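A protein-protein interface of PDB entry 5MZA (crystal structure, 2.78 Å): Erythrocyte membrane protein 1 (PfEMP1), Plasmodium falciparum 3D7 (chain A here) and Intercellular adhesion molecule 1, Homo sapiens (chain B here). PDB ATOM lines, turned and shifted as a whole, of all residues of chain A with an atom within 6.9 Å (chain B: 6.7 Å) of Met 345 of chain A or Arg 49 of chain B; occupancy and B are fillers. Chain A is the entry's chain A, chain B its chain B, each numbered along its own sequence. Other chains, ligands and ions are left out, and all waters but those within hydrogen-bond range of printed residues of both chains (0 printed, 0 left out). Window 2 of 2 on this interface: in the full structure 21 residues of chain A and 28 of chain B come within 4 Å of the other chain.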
ATOM      1  N   ASP A 106      12.480  14.262  30.281  1.00  0.00           N
ATOM      2  CA  ASP A 106      13.260  15.410  30.774  1.00  0.00           C
ATOM      3  C   ASP A 106      12.479  16.299  31.767  1.00  0.00           C
ATOM      4  O   ASP A 106      12.616  17.528  31.775  1.00  0.00           O
ATOM      5  CB  ASP A 106      13.858  16.207  29.598  1.00  0.00           C
ATOM      6  CG  ASP A 106      14.639  15.321  28.642  1.00  0.00           C
ATOM      7  OD1 ASP A 106      15.719  14.821  29.041  1.00  0.00           O
ATOM      8  OD2 ASP A 106      14.140  15.071  27.523  1.00  0.00           O
ATOM      9  N   SER A 340      16.924  22.430  28.682  1.00  0.00           N
ATOM     10  CA  SER A 340      17.165  23.308  27.525  1.00  0.00           C
ATOM     11  C   SER A 340      16.839  22.629  26.197  1.00  0.00           C
ATOM     12  O   SER A 340      16.075  23.179  25.401  1.00  0.00           O
ATOM     13  CB  SER A 340      18.613  23.793  27.499  1.00  0.00           C
ATOM     14  OG  SER A 340      18.968  24.483  28.682  1.00  0.00           O
ATOM     15  N   TYR A 341      17.425  21.438  25.968  1.00  0.00           N
ATOM     16  CA  TYR A 341      17.262  20.661  24.744  1.00  0.00           C
ATOM     17  C   TYR A 341      15.837  20.128  24.552  1.00  0.00           C
ATOM     18  O   TYR A 341      15.425  19.937  23.407  1.00  0.00           O
ATOM     19  CB  TYR A 341      18.315  19.542  24.645  1.00  0.00           C
ATOM     20  CG  TYR A 341      19.749  20.035  24.529  1.00  0.00           C
ATOM     21  CD1 TYR A 341      20.164  20.786  23.431  1.00  0.00           C
ATOM     22  CD2 TYR A 341      20.708  19.676  25.473  1.00  0.00           C
ATOM     23  CE1 TYR A 341      21.486  21.213  23.304  1.00  0.00           C
ATOM     24  CE2 TYR A 341      22.033  20.098  25.357  1.00  0.00           C
ATOM     25  CZ  TYR A 341      22.419  20.863  24.268  1.00  0.00           C
ATOM     26  OH  TYR A 341      23.724  21.276  24.151  1.00  0.00           O
ATOM     27  N   LYS A 342      15.072  19.931  25.647  1.00  0.00           N
ATOM     28  CA  LYS A 342      13.675  19.513  25.547  1.00  0.00           C
ATOM     29  C   LYS A 342      12.847  20.730  25.130  1.00  0.00           C
ATOM     30  O   LYS A 342      12.071  20.642  24.177  1.00  0.00           O
ATOM     31  CB  LYS A 342      13.151  18.916  26.872  1.00  0.00           C
ATOM     32  CG  LYS A 342      11.724  18.343  26.795  1.00  0.00           C
ATOM     33  CD  LYS A 342      11.651  17.035  26.002  1.00  0.00           C
ATOM     34  CE  LYS A 342      10.243  16.550  25.820  1.00  0.00           C
ATOM     35  NZ  LYS A 342      10.201  15.332  24.976  1.00  0.00           N
ATOM     36  N   TYR A 343      13.048  21.875  25.820  1.00  0.00           N
ATOM     37  CA  TYR A 343      12.371  23.143  25.539  1.00  0.00           C
ATOM     38  C   TYR A 343      12.606  23.576  24.084  1.00  0.00           C
ATOM     39  O   TYR A 343      11.674  24.067  23.441  1.00  0.00           O
ATOM     40  CB  TYR A 343      12.841  24.240  26.513  1.00  0.00           C
ATOM     41  CG  TYR A 343      12.162  25.574  26.296  1.00  0.00           C
ATOM     42  CD1 TYR A 343      12.682  26.509  25.406  1.00  0.00           C
ATOM     43  CD2 TYR A 343      10.983  25.894  26.963  1.00  0.00           C
ATOM     44  CE1 TYR A 343      12.043  27.725  25.179  1.00  0.00           C
ATOM     45  CE2 TYR A 343      10.343  27.115  26.754  1.00  0.00           C
ATOM     46  CZ  TYR A 343      10.878  28.028  25.861  1.00  0.00           C
ATOM     47  OH  TYR A 343      10.254  29.230  25.652  1.00  0.00           O
ATOM     48  N   LEU A 344      13.854  23.396  23.583  1.00  0.00           N
ATOM     49  CA  LEU A 344      14.273  23.730  22.221  1.00  0.00           C
ATOM     50  C   LEU A 344      13.442  22.951  21.207  1.00  0.00           C
ATOM     51  O   LEU A 344      12.943  23.537  20.243  1.00  0.00           O
ATOM     52  CB  LEU A 344      15.770  23.441  22.042  1.00  0.00           C
ATOM     53  CG  LEU A 344      16.471  24.165  20.892  1.00  0.00           C
ATOM     54  CD1 LEU A 344      16.705  25.641  21.225  1.00  0.00           C
ATOM     55  CD2 LEU A 344      17.781  23.485  20.547  1.00  0.00           C
ATOM     56  N   MET A 345      13.244  21.643  21.470  1.00  0.00           N
ATOM     57  CA  MET A 345      12.428  20.747  20.654  1.00  0.00           C
ATOM     58  C   MET A 345      10.964  21.183  20.680  1.00  0.00           C
ATOM     59  O   MET A 345      10.343  21.295  19.624  1.00  0.00           O
ATOM     60  CB  MET A 345      12.555  19.299  21.151  1.00  0.00           C
ATOM     61  CG  MET A 345      13.839  18.624  20.725  1.00  0.00           C
ATOM     62  SD  MET A 345      13.922  18.287  18.948  1.00  0.00           S
ATOM     63  CE  MET A 345      12.883  16.824  18.850  1.00  0.00           C
ATOM     64  N   LEU A 346      10.427  21.460  21.880  1.00  0.00           N
ATOM     65  CA  LEU A 346       9.037  21.875  22.061  1.00  0.00           C
ATOM     66  C   LEU A 346       8.725  23.216  21.412  1.00  0.00           C
ATOM     67  O   LEU A 346       7.644  23.367  20.844  1.00  0.00           O
ATOM     68  CB  LEU A 346       8.629  21.864  23.543  1.00  0.00           C
ATOM     69  CG  LEU A 346       8.692  20.521  24.263  1.00  0.00           C
ATOM     70  CD1 LEU A 346       8.457  20.692  25.755  1.00  0.00           C
ATOM     71  CD2 LEU A 346       7.718  19.508  23.669  1.00  0.00           C
ATOM     72  N   TYR A 347       9.670  24.177  21.480  1.00  0.00           N
ATOM     73  CA  TYR A 347       9.505  25.501  20.873  1.00  0.00           C
ATOM     74  C   TYR A 347       9.540  25.391  19.341  1.00  0.00           C
ATOM     75  O   TYR A 347       8.773  26.081  18.668  1.00  0.00           O
ATOM     76  CB  TYR A 347      10.562  26.503  21.390  1.00  0.00           C
ATOM     77  CG  TYR A 347      10.301  27.929  20.951  1.00  0.00           C
ATOM     78  CD1 TYR A 347      10.844  28.427  19.768  1.00  0.00           C
ATOM     79  CD2 TYR A 347       9.498  28.778  21.708  1.00  0.00           C
ATOM     80  CE1 TYR A 347      10.582  29.728  19.343  1.00  0.00           C
ATOM     81  CE2 TYR A 347       9.237  30.085  21.297  1.00  0.00           C
ATOM     82  CZ  TYR A 347       9.788  30.557  20.116  1.00  0.00           C
ATOM     83  OH  TYR A 347       9.539  31.842  19.706  1.00  0.00           O
ATOM     84  N   ALA A 348      10.423  24.524  18.803  1.00  0.00           N
ATOM     85  CA  ALA A 348      10.551  24.269  17.363  1.00  0.00           C
ATOM     86  C   ALA A 348       9.239  23.706  16.827  1.00  0.00           C
ATOM     87  O   ALA A 348       8.767  24.159  15.788  1.00  0.00           O
ATOM     88  CB  ALA A 348      11.690  23.294  17.100  1.00  0.00           C
ATOM     89  N   LYS A 349       8.627  22.762  17.576  1.00  0.00           N
ATOM     90  CA  LYS A 349       7.349  22.127  17.259  1.00  0.00           C
ATOM     91  C   LYS A 349       6.230  23.165  17.225  1.00  0.00           C
ATOM     92  O   LYS A 349       5.396  23.131  16.321  1.00  0.00           O
ATOM     93  CB  LYS A 349       7.030  21.018  18.272  1.00  0.00           C
ATOM     94  CG  LYS A 349       7.830  19.738  18.063  1.00  0.00           C
ATOM     95  CD  LYS A 349       7.568  18.739  19.187  1.00  0.00           C
ATOM     96  CE  LYS A 349       8.512  17.559  19.179  1.00  0.00           C
ATOM     97  NZ  LYS A 349       8.246  16.635  18.046  1.00  0.00           N
ATOM     98  N   ALA A 350       6.250  24.108  18.186  1.00  0.00           N
ATOM     99  CA  ALA A 350       5.287  25.204  18.321  1.00  0.00           C
ATOM    100  C   ALA A 350       5.423  26.190  17.165  1.00  0.00           C
ATOM    101  O   ALA A 350       4.417  26.579  16.570  1.00  0.00           O
ATOM    102  CB  ALA A 350       5.499  25.914  19.645  1.00  0.00           C
ATOM    103  N   ILE A 352       6.827  25.563  14.188  1.00  0.00           N
ATOM    104  CA  ILE A 352       6.446  24.848  12.961  1.00  0.00           C
ATOM    105  C   ILE A 352       4.912  24.832  12.818  1.00  0.00           C
ATOM    106  O   ILE A 352       4.410  25.112  11.727  1.00  0.00           O
ATOM    107  CB  ILE A 352       7.121  23.444  12.853  1.00  0.00           C
ATOM    108  CG1 ILE A 352       8.620  23.600  12.500  1.00  0.00           C
ATOM    109  CG2 ILE A 352       6.417  22.534  11.830  1.00  0.00           C
ATOM    110  CD1 ILE A 352       9.493  22.465  12.906  1.00  0.00           C
ATOM    111  N   VAL A 374       3.280  22.749  23.918  1.00  0.00           N
ATOM    112  CA  VAL A 374       3.438  23.111  22.505  1.00  0.00           C
ATOM    113  C   VAL A 374       2.390  24.190  22.148  1.00  0.00           C
ATOM    114  O   VAL A 374       2.724  25.150  21.456  1.00  0.00           O
ATOM    115  CB  VAL A 374       3.416  21.868  21.559  1.00  0.00           C
ATOM    116  CG1 VAL A 374       3.461  22.275  20.084  1.00  0.00           C
ATOM    117  CG2 VAL A 374       4.566  20.911  21.876  1.00  0.00           C
ATOM    118  N   LEU A 377       3.481  27.620  23.973  1.00  0.00           N
ATOM    119  CA  LEU A 377       4.630  28.170  23.255  1.00  0.00           C
ATOM    120  C   LEU A 377       4.259  28.644  21.842  1.00  0.00           C
ATOM    121  O   LEU A 377       4.922  29.533  21.303  1.00  0.00           O
ATOM    122  CB  LEU A 377       5.795  27.165  23.215  1.00  0.00           C
ATOM    123  CG  LEU A 377       6.407  26.738  24.559  1.00  0.00           C
ATOM    124  CD1 LEU A 377       7.325  25.541  24.384  1.00  0.00           C
ATOM    125  CD2 LEU A 377       7.135  27.881  25.235  1.00  0.00           C
ATOM    126  N   LEU B  18       9.427  18.740  11.372  1.00  0.00           N
ATOM    127  CA  LEU B  18      10.552  18.398  12.228  1.00  0.00           C
ATOM    128  C   LEU B  18      10.738  16.884  12.153  1.00  0.00           C
ATOM    129  O   LEU B  18       9.857  16.132  12.582  1.00  0.00           O
ATOM    130  CB  LEU B  18      10.271  18.863  13.671  1.00  0.00           C
ATOM    131  CG  LEU B  18      11.480  19.068  14.575  1.00  0.00           C
ATOM    132  CD1 LEU B  18      12.261  20.322  14.188  1.00  0.00           C
ATOM    133  CD2 LEU B  18      11.064  19.141  16.031  1.00  0.00           C
ATOM    134  N   THR B  20      13.272  13.444  12.915  1.00  0.00           N
ATOM    135  CA  THR B  20      14.327  12.910  13.778  1.00  0.00           C
ATOM    136  C   THR B  20      14.868  11.579  13.254  1.00  0.00           C
ATOM    137  O   THR B  20      14.189  10.552  13.345  1.00  0.00           O
ATOM    138  CB  THR B  20      13.858  12.824  15.247  1.00  0.00           C
ATOM    139  OG1 THR B  20      13.360  14.089  15.672  1.00  0.00           O
ATOM    140  CG2 THR B  20      14.959  12.371  16.195  1.00  0.00           C
ATOM    141  N   CYS B  21      16.105  11.605  12.724  1.00  0.00           N
ATOM    142  CA  CYS B  21      16.813  10.416  12.248  1.00  0.00           C
ATOM    143  C   CYS B  21      17.552   9.851  13.458  1.00  0.00           C
ATOM    144  O   CYS B  21      18.263  10.594  14.139  1.00  0.00           O
ATOM    145  CB  CYS B  21      17.784  10.762  11.122  1.00  0.00           C
ATOM    146  SG  CYS B  21      17.031  11.610   9.711  1.00  0.00           S
ATOM    147  N   SER B  22      17.360   8.555  13.747  1.00  0.00           N
ATOM    148  CA  SER B  22      17.996   7.874  14.878  1.00  0.00           C
ATOM    149  C   SER B  22      18.527   6.489  14.496  1.00  0.00           C
ATOM    150  O   SER B  22      17.964   5.833  13.618  1.00  0.00           O
ATOM    151  CB  SER B  22      17.034   7.777  16.059  1.00  0.00           C
ATOM    152  OG  SER B  22      16.852   9.039  16.682  1.00  0.00           O
ATOM    153  N   THR B  23      19.615   6.051  15.158  1.00  0.00           N
ATOM    154  CA  THR B  23      20.237   4.751  14.892  1.00  0.00           C
ATOM    155  C   THR B  23      20.436   3.927  16.177  1.00  0.00           C
ATOM    156  O   THR B  23      20.623   4.490  17.261  1.00  0.00           O
ATOM    157  CB  THR B  23      21.526   4.917  14.059  1.00  0.00           C
ATOM    158  OG1 THR B  23      22.025   3.628  13.695  1.00  0.00           O
ATOM    159  CG2 THR B  23      22.605   5.727  14.771  1.00  0.00           C
ATOM    160  N   PRO B  28      28.055   5.925  15.586  1.00  0.00           N
ATOM    161  CA  PRO B  28      28.099   5.629  14.143  1.00  0.00           C
ATOM    162  C   PRO B  28      29.060   6.545  13.381  1.00  0.00           C
ATOM    163  O   PRO B  28      29.301   7.680  13.804  1.00  0.00           O
ATOM    164  CB  PRO B  28      26.650   5.827  13.699  1.00  0.00           C
ATOM    165  CG  PRO B  28      26.104   6.842  14.647  1.00  0.00           C
ATOM    166  CD  PRO B  28      26.888   6.766  15.931  1.00  0.00           C
ATOM    167  N   LEU B  31      25.756   9.694   9.739  1.00  0.00           N
ATOM    168  CA  LEU B  31      24.364   9.913  10.138  1.00  0.00           C
ATOM    169  C   LEU B  31      23.893  11.216   9.504  1.00  0.00           C
ATOM    170  O   LEU B  31      24.483  12.276   9.745  1.00  0.00           O
ATOM    171  CB  LEU B  31      24.200   9.940  11.682  1.00  0.00           C
ATOM    172  CG  LEU B  31      22.777  10.100  12.250  1.00  0.00           C
ATOM    173  CD1 LEU B  31      21.948   8.838  12.062  1.00  0.00           C
ATOM    174  CD2 LEU B  31      22.818  10.446  13.715  1.00  0.00           C
ATOM    175  N   GLU B  41      19.597  21.755  10.661  1.00  0.00           N
ATOM    176  CA  GLU B  41      19.824  20.745  11.686  1.00  0.00           C
ATOM    177  C   GLU B  41      19.823  21.379  13.073  1.00  0.00           C
ATOM    178  O   GLU B  41      20.575  22.325  13.317  1.00  0.00           O
ATOM    179  CB  GLU B  41      21.132  19.979  11.420  1.00  0.00           C
ATOM    180  CG  GLU B  41      21.299  18.725  12.264  1.00  0.00           C
ATOM    181  CD  GLU B  41      22.698  18.143  12.304  1.00  0.00           C
ATOM    182  OE1 GLU B  41      23.344  18.042  11.235  1.00  0.00           O
ATOM    183  OE2 GLU B  41      23.138  17.754  13.410  1.00  0.00           O
ATOM    184  N   LEU B  42      18.957  20.871  13.968  1.00  0.00           N
ATOM    185  CA  LEU B  42      18.866  21.337  15.349  1.00  0.00           C
ATOM    186  C   LEU B  42      19.914  20.615  16.177  1.00  0.00           C
ATOM    187  O   LEU B  42      19.865  19.388  16.310  1.00  0.00           O
ATOM    188  CB  LEU B  42      17.462  21.127  15.932  1.00  0.00           C
ATOM    189  CG  LEU B  42      16.436  22.212  15.635  1.00  0.00           C
ATOM    190  CD1 LEU B  42      15.063  21.765  16.057  1.00  0.00           C
ATOM    191  CD2 LEU B  42      16.782  23.527  16.351  1.00  0.00           C
ATOM    192  N   LEU B  44      21.848  18.998  18.987  1.00  0.00           N
ATOM    193  CA  LEU B  44      21.508  18.239  20.190  1.00  0.00           C
ATOM    194  C   LEU B  44      22.714  17.455  20.742  1.00  0.00           C
ATOM    195  O   LEU B  44      23.675  17.248  19.999  1.00  0.00           O
ATOM    196  CB  LEU B  44      20.321  17.296  19.906  1.00  0.00           C
ATOM    197  CG  LEU B  44      18.946  17.929  19.637  1.00  0.00           C
ATOM    198  CD1 LEU B  44      17.905  16.868  19.532  1.00  0.00           C
ATOM    199  CD2 LEU B  44      18.523  18.884  20.748  1.00  0.00           C
ATOM    200  N   PRO B  45      22.706  17.016  22.028  1.00  0.00           N
ATOM    201  CA  PRO B  45      23.875  16.286  22.556  1.00  0.00           C
ATOM    202  C   PRO B  45      24.093  14.890  21.969  1.00  0.00           C
ATOM    203  O   PRO B  45      25.232  14.418  21.939  1.00  0.00           O
ATOM    204  CB  PRO B  45      23.609  16.231  24.062  1.00  0.00           C
ATOM    205  CG  PRO B  45      22.131  16.310  24.188  1.00  0.00           C
ATOM    206  CD  PRO B  45      21.664  17.184  23.065  1.00  0.00           C
ATOM    207  N   GLY B  46      23.011  14.257  21.516  1.00  0.00           N
ATOM    208  CA  GLY B  46      23.029  12.918  20.937  1.00  0.00           C
ATOM    209  C   GLY B  46      23.903  12.770  19.706  1.00  0.00           C
ATOM    210  O   GLY B  46      23.846  13.603  18.795  1.00  0.00           O
ATOM    211  N   ASN B  47      24.728  11.704  19.683  1.00  0.00           N
ATOM    212  CA  ASN B  47      25.623  11.384  18.568  1.00  0.00           C
ATOM    213  C   ASN B  47      25.014  10.322  17.636  1.00  0.00           C
ATOM    214  O   ASN B  47      25.511  10.116  16.527  1.00  0.00           O
ATOM    215  CB  ASN B  47      26.992  10.936  19.091  1.00  0.00           C
ATOM    216  CG  ASN B  47      28.176  11.555  18.381  1.00  0.00           C
ATOM    217  OD1 ASN B  47      28.046  12.423  17.503  1.00  0.00           O
ATOM    218  ND2 ASN B  47      29.368  11.128  18.766  1.00  0.00           N
ATOM    219  N   ASN B  48      23.927   9.664  18.096  1.00  0.00           N
ATOM    220  CA  ASN B  48      23.181   8.625  17.379  1.00  0.00           C
ATOM    221  C   ASN B  48      21.759   9.101  16.995  1.00  0.00           C
ATOM    222  O   ASN B  48      20.951   8.310  16.498  1.00  0.00           O
ATOM    223  CB  ASN B  48      23.121   7.344  18.233  1.00  0.00           C
ATOM    224  CG  ASN B  48      22.337   7.454  19.527  1.00  0.00           C
ATOM    225  OD1 ASN B  48      22.310   8.496  20.200  1.00  0.00           O
ATOM    226  ND2 ASN B  48      21.706   6.359  19.922  1.00  0.00           N
ATOM    227  N   ARG B  49      21.476  10.397  17.215  1.00  0.00           N
ATOM    228  CA  ARG B  49      20.187  11.042  16.962  1.00  0.00           C
ATOM    229  C   ARG B  49      20.416  12.436  16.358  1.00  0.00           C
ATOM    230  O   ARG B  49      21.222  13.206  16.886  1.00  0.00           O
ATOM    231  CB  ARG B  49      19.416  11.139  18.296  1.00  0.00           C
ATOM    232  CG  ARG B  49      18.088  11.878  18.248  1.00  0.00           C
ATOM    233  CD  ARG B  49      17.823  12.586  19.562  1.00  0.00           C
ATOM    234  NE  ARG B  49      16.480  13.165  19.608  1.00  0.00           N
ATOM    235  CZ  ARG B  49      16.020  13.925  20.599  1.00  0.00           C
ATOM    236  NH1 ARG B  49      14.784  14.405  20.555  1.00  0.00           N
ATOM    237  NH2 ARG B  49      16.795  14.214  21.638  1.00  0.00           N
ATOM    238  N   LYS B  50      19.705  12.760  15.265  1.00  0.00           N
ATOM    239  CA  LYS B  50      19.813  14.065  14.607  1.00  0.00           C
ATOM    240  C   LYS B  50      18.449  14.634  14.216  1.00  0.00           C
ATOM    241  O   LYS B  50      17.666  13.960  13.545  1.00  0.00           O
ATOM    242  CB  LYS B  50      20.790  14.024  13.419  1.00  0.00           C
ATOM    243  CG  LYS B  50      22.232  14.284  13.839  1.00  0.00           C
ATOM    244  CD  LYS B  50      23.226  14.137  12.700  1.00  0.00           C
ATOM    245  CE  LYS B  50      24.631  14.388  13.185  1.00  0.00           C
ATOM    246  NZ  LYS B  50      25.644  13.999  12.171  1.00  0.00           N
ATOM    247  N   VAL B  51      18.166  15.869  14.651  1.00  0.00           N
ATOM    248  CA  VAL B  51      16.898  16.547  14.379  1.00  0.00           C
ATOM    249  C   VAL B  51      17.052  17.560  13.243  1.00  0.00           C
ATOM    250  O   VAL B  51      17.981  18.364  13.259  1.00  0.00           O
ATOM    251  CB  VAL B  51      16.280  17.149  15.669  1.00  0.00           C
ATOM    252  CG1 VAL B  51      15.015  17.951  15.367  1.00  0.00           C
ATOM    253  CG2 VAL B  51      15.973  16.045  16.676  1.00  0.00           C
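Of chain B, only Arg 49 (3.5 Å) and Val 51 (3.8 Å) come within 4 Å of Met 345 of chain A.
Of the printed residues of chain A, Leu 18 of chain B touches Lys 349 (3.9 Å) and Ile 352 (3.7 Å).
Printed residues of chain A within 4 Å of Leu 42 of chain B: Ala 348 (3.8 Å).
Printed residues of chain A within 4 Å of Pro 45 of chain B: Tyr 341 (3.6 Å).
Arg 49 of chain B touches just one residue of chain A: Met 345.
Printed residues of chain A within 4 Å of Val 51 of chain B: Met 345.
The nearest residue of chain B that does not touch Met 345 of chain A is Leu 18 of chain B (4.1 Å).
The nearest printed residue of chain A that does not touch Leu 18 of chain B is Met 345 of chain A (4.1 Å).
N of Leu 42 of chain B lies within hydrogen-bond range of O of Val 51 of chain B (2.8 Å).
Of the 17 printed residues of chain B, 6 touch a printed residue of chain A.
Printed residues of chain B that touch a printed residue of chain A: Leu 18, Leu 42, Leu 44, Pro 45, Arg 49 and Val 51.
Hydrophobic or aromatic side chains of chain B that line the printed part of chain A: Leu 18, Leu 42, Leu 44, Pro 45 and Val 51.
Of the 15 printed residues of chain A, 5 touch a printed residue of chain B.
Among the printed residues, 7 pairs touch across the chains.
Among the printed residues, no Asp or Glu carboxylate lies within 4 Å of a Lys or Arg side-chain nitrogen of the other chain.
Among the printed residues, pairs that only touch across the chains: Tyr 341 of chain A with Leu 44 of chain B, Tyr 341 of chain A with Pro 45 of chain B, Met 345 of chain A with Arg 49 of chain B, Met 345 of chain A with Val 51 of chain B, Ala 348 of chain A with Leu 42 of chain B, Lys 349 of chain A with Leu 18 of chain B and Ile 352 of chain A with Leu 18 of chain B.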
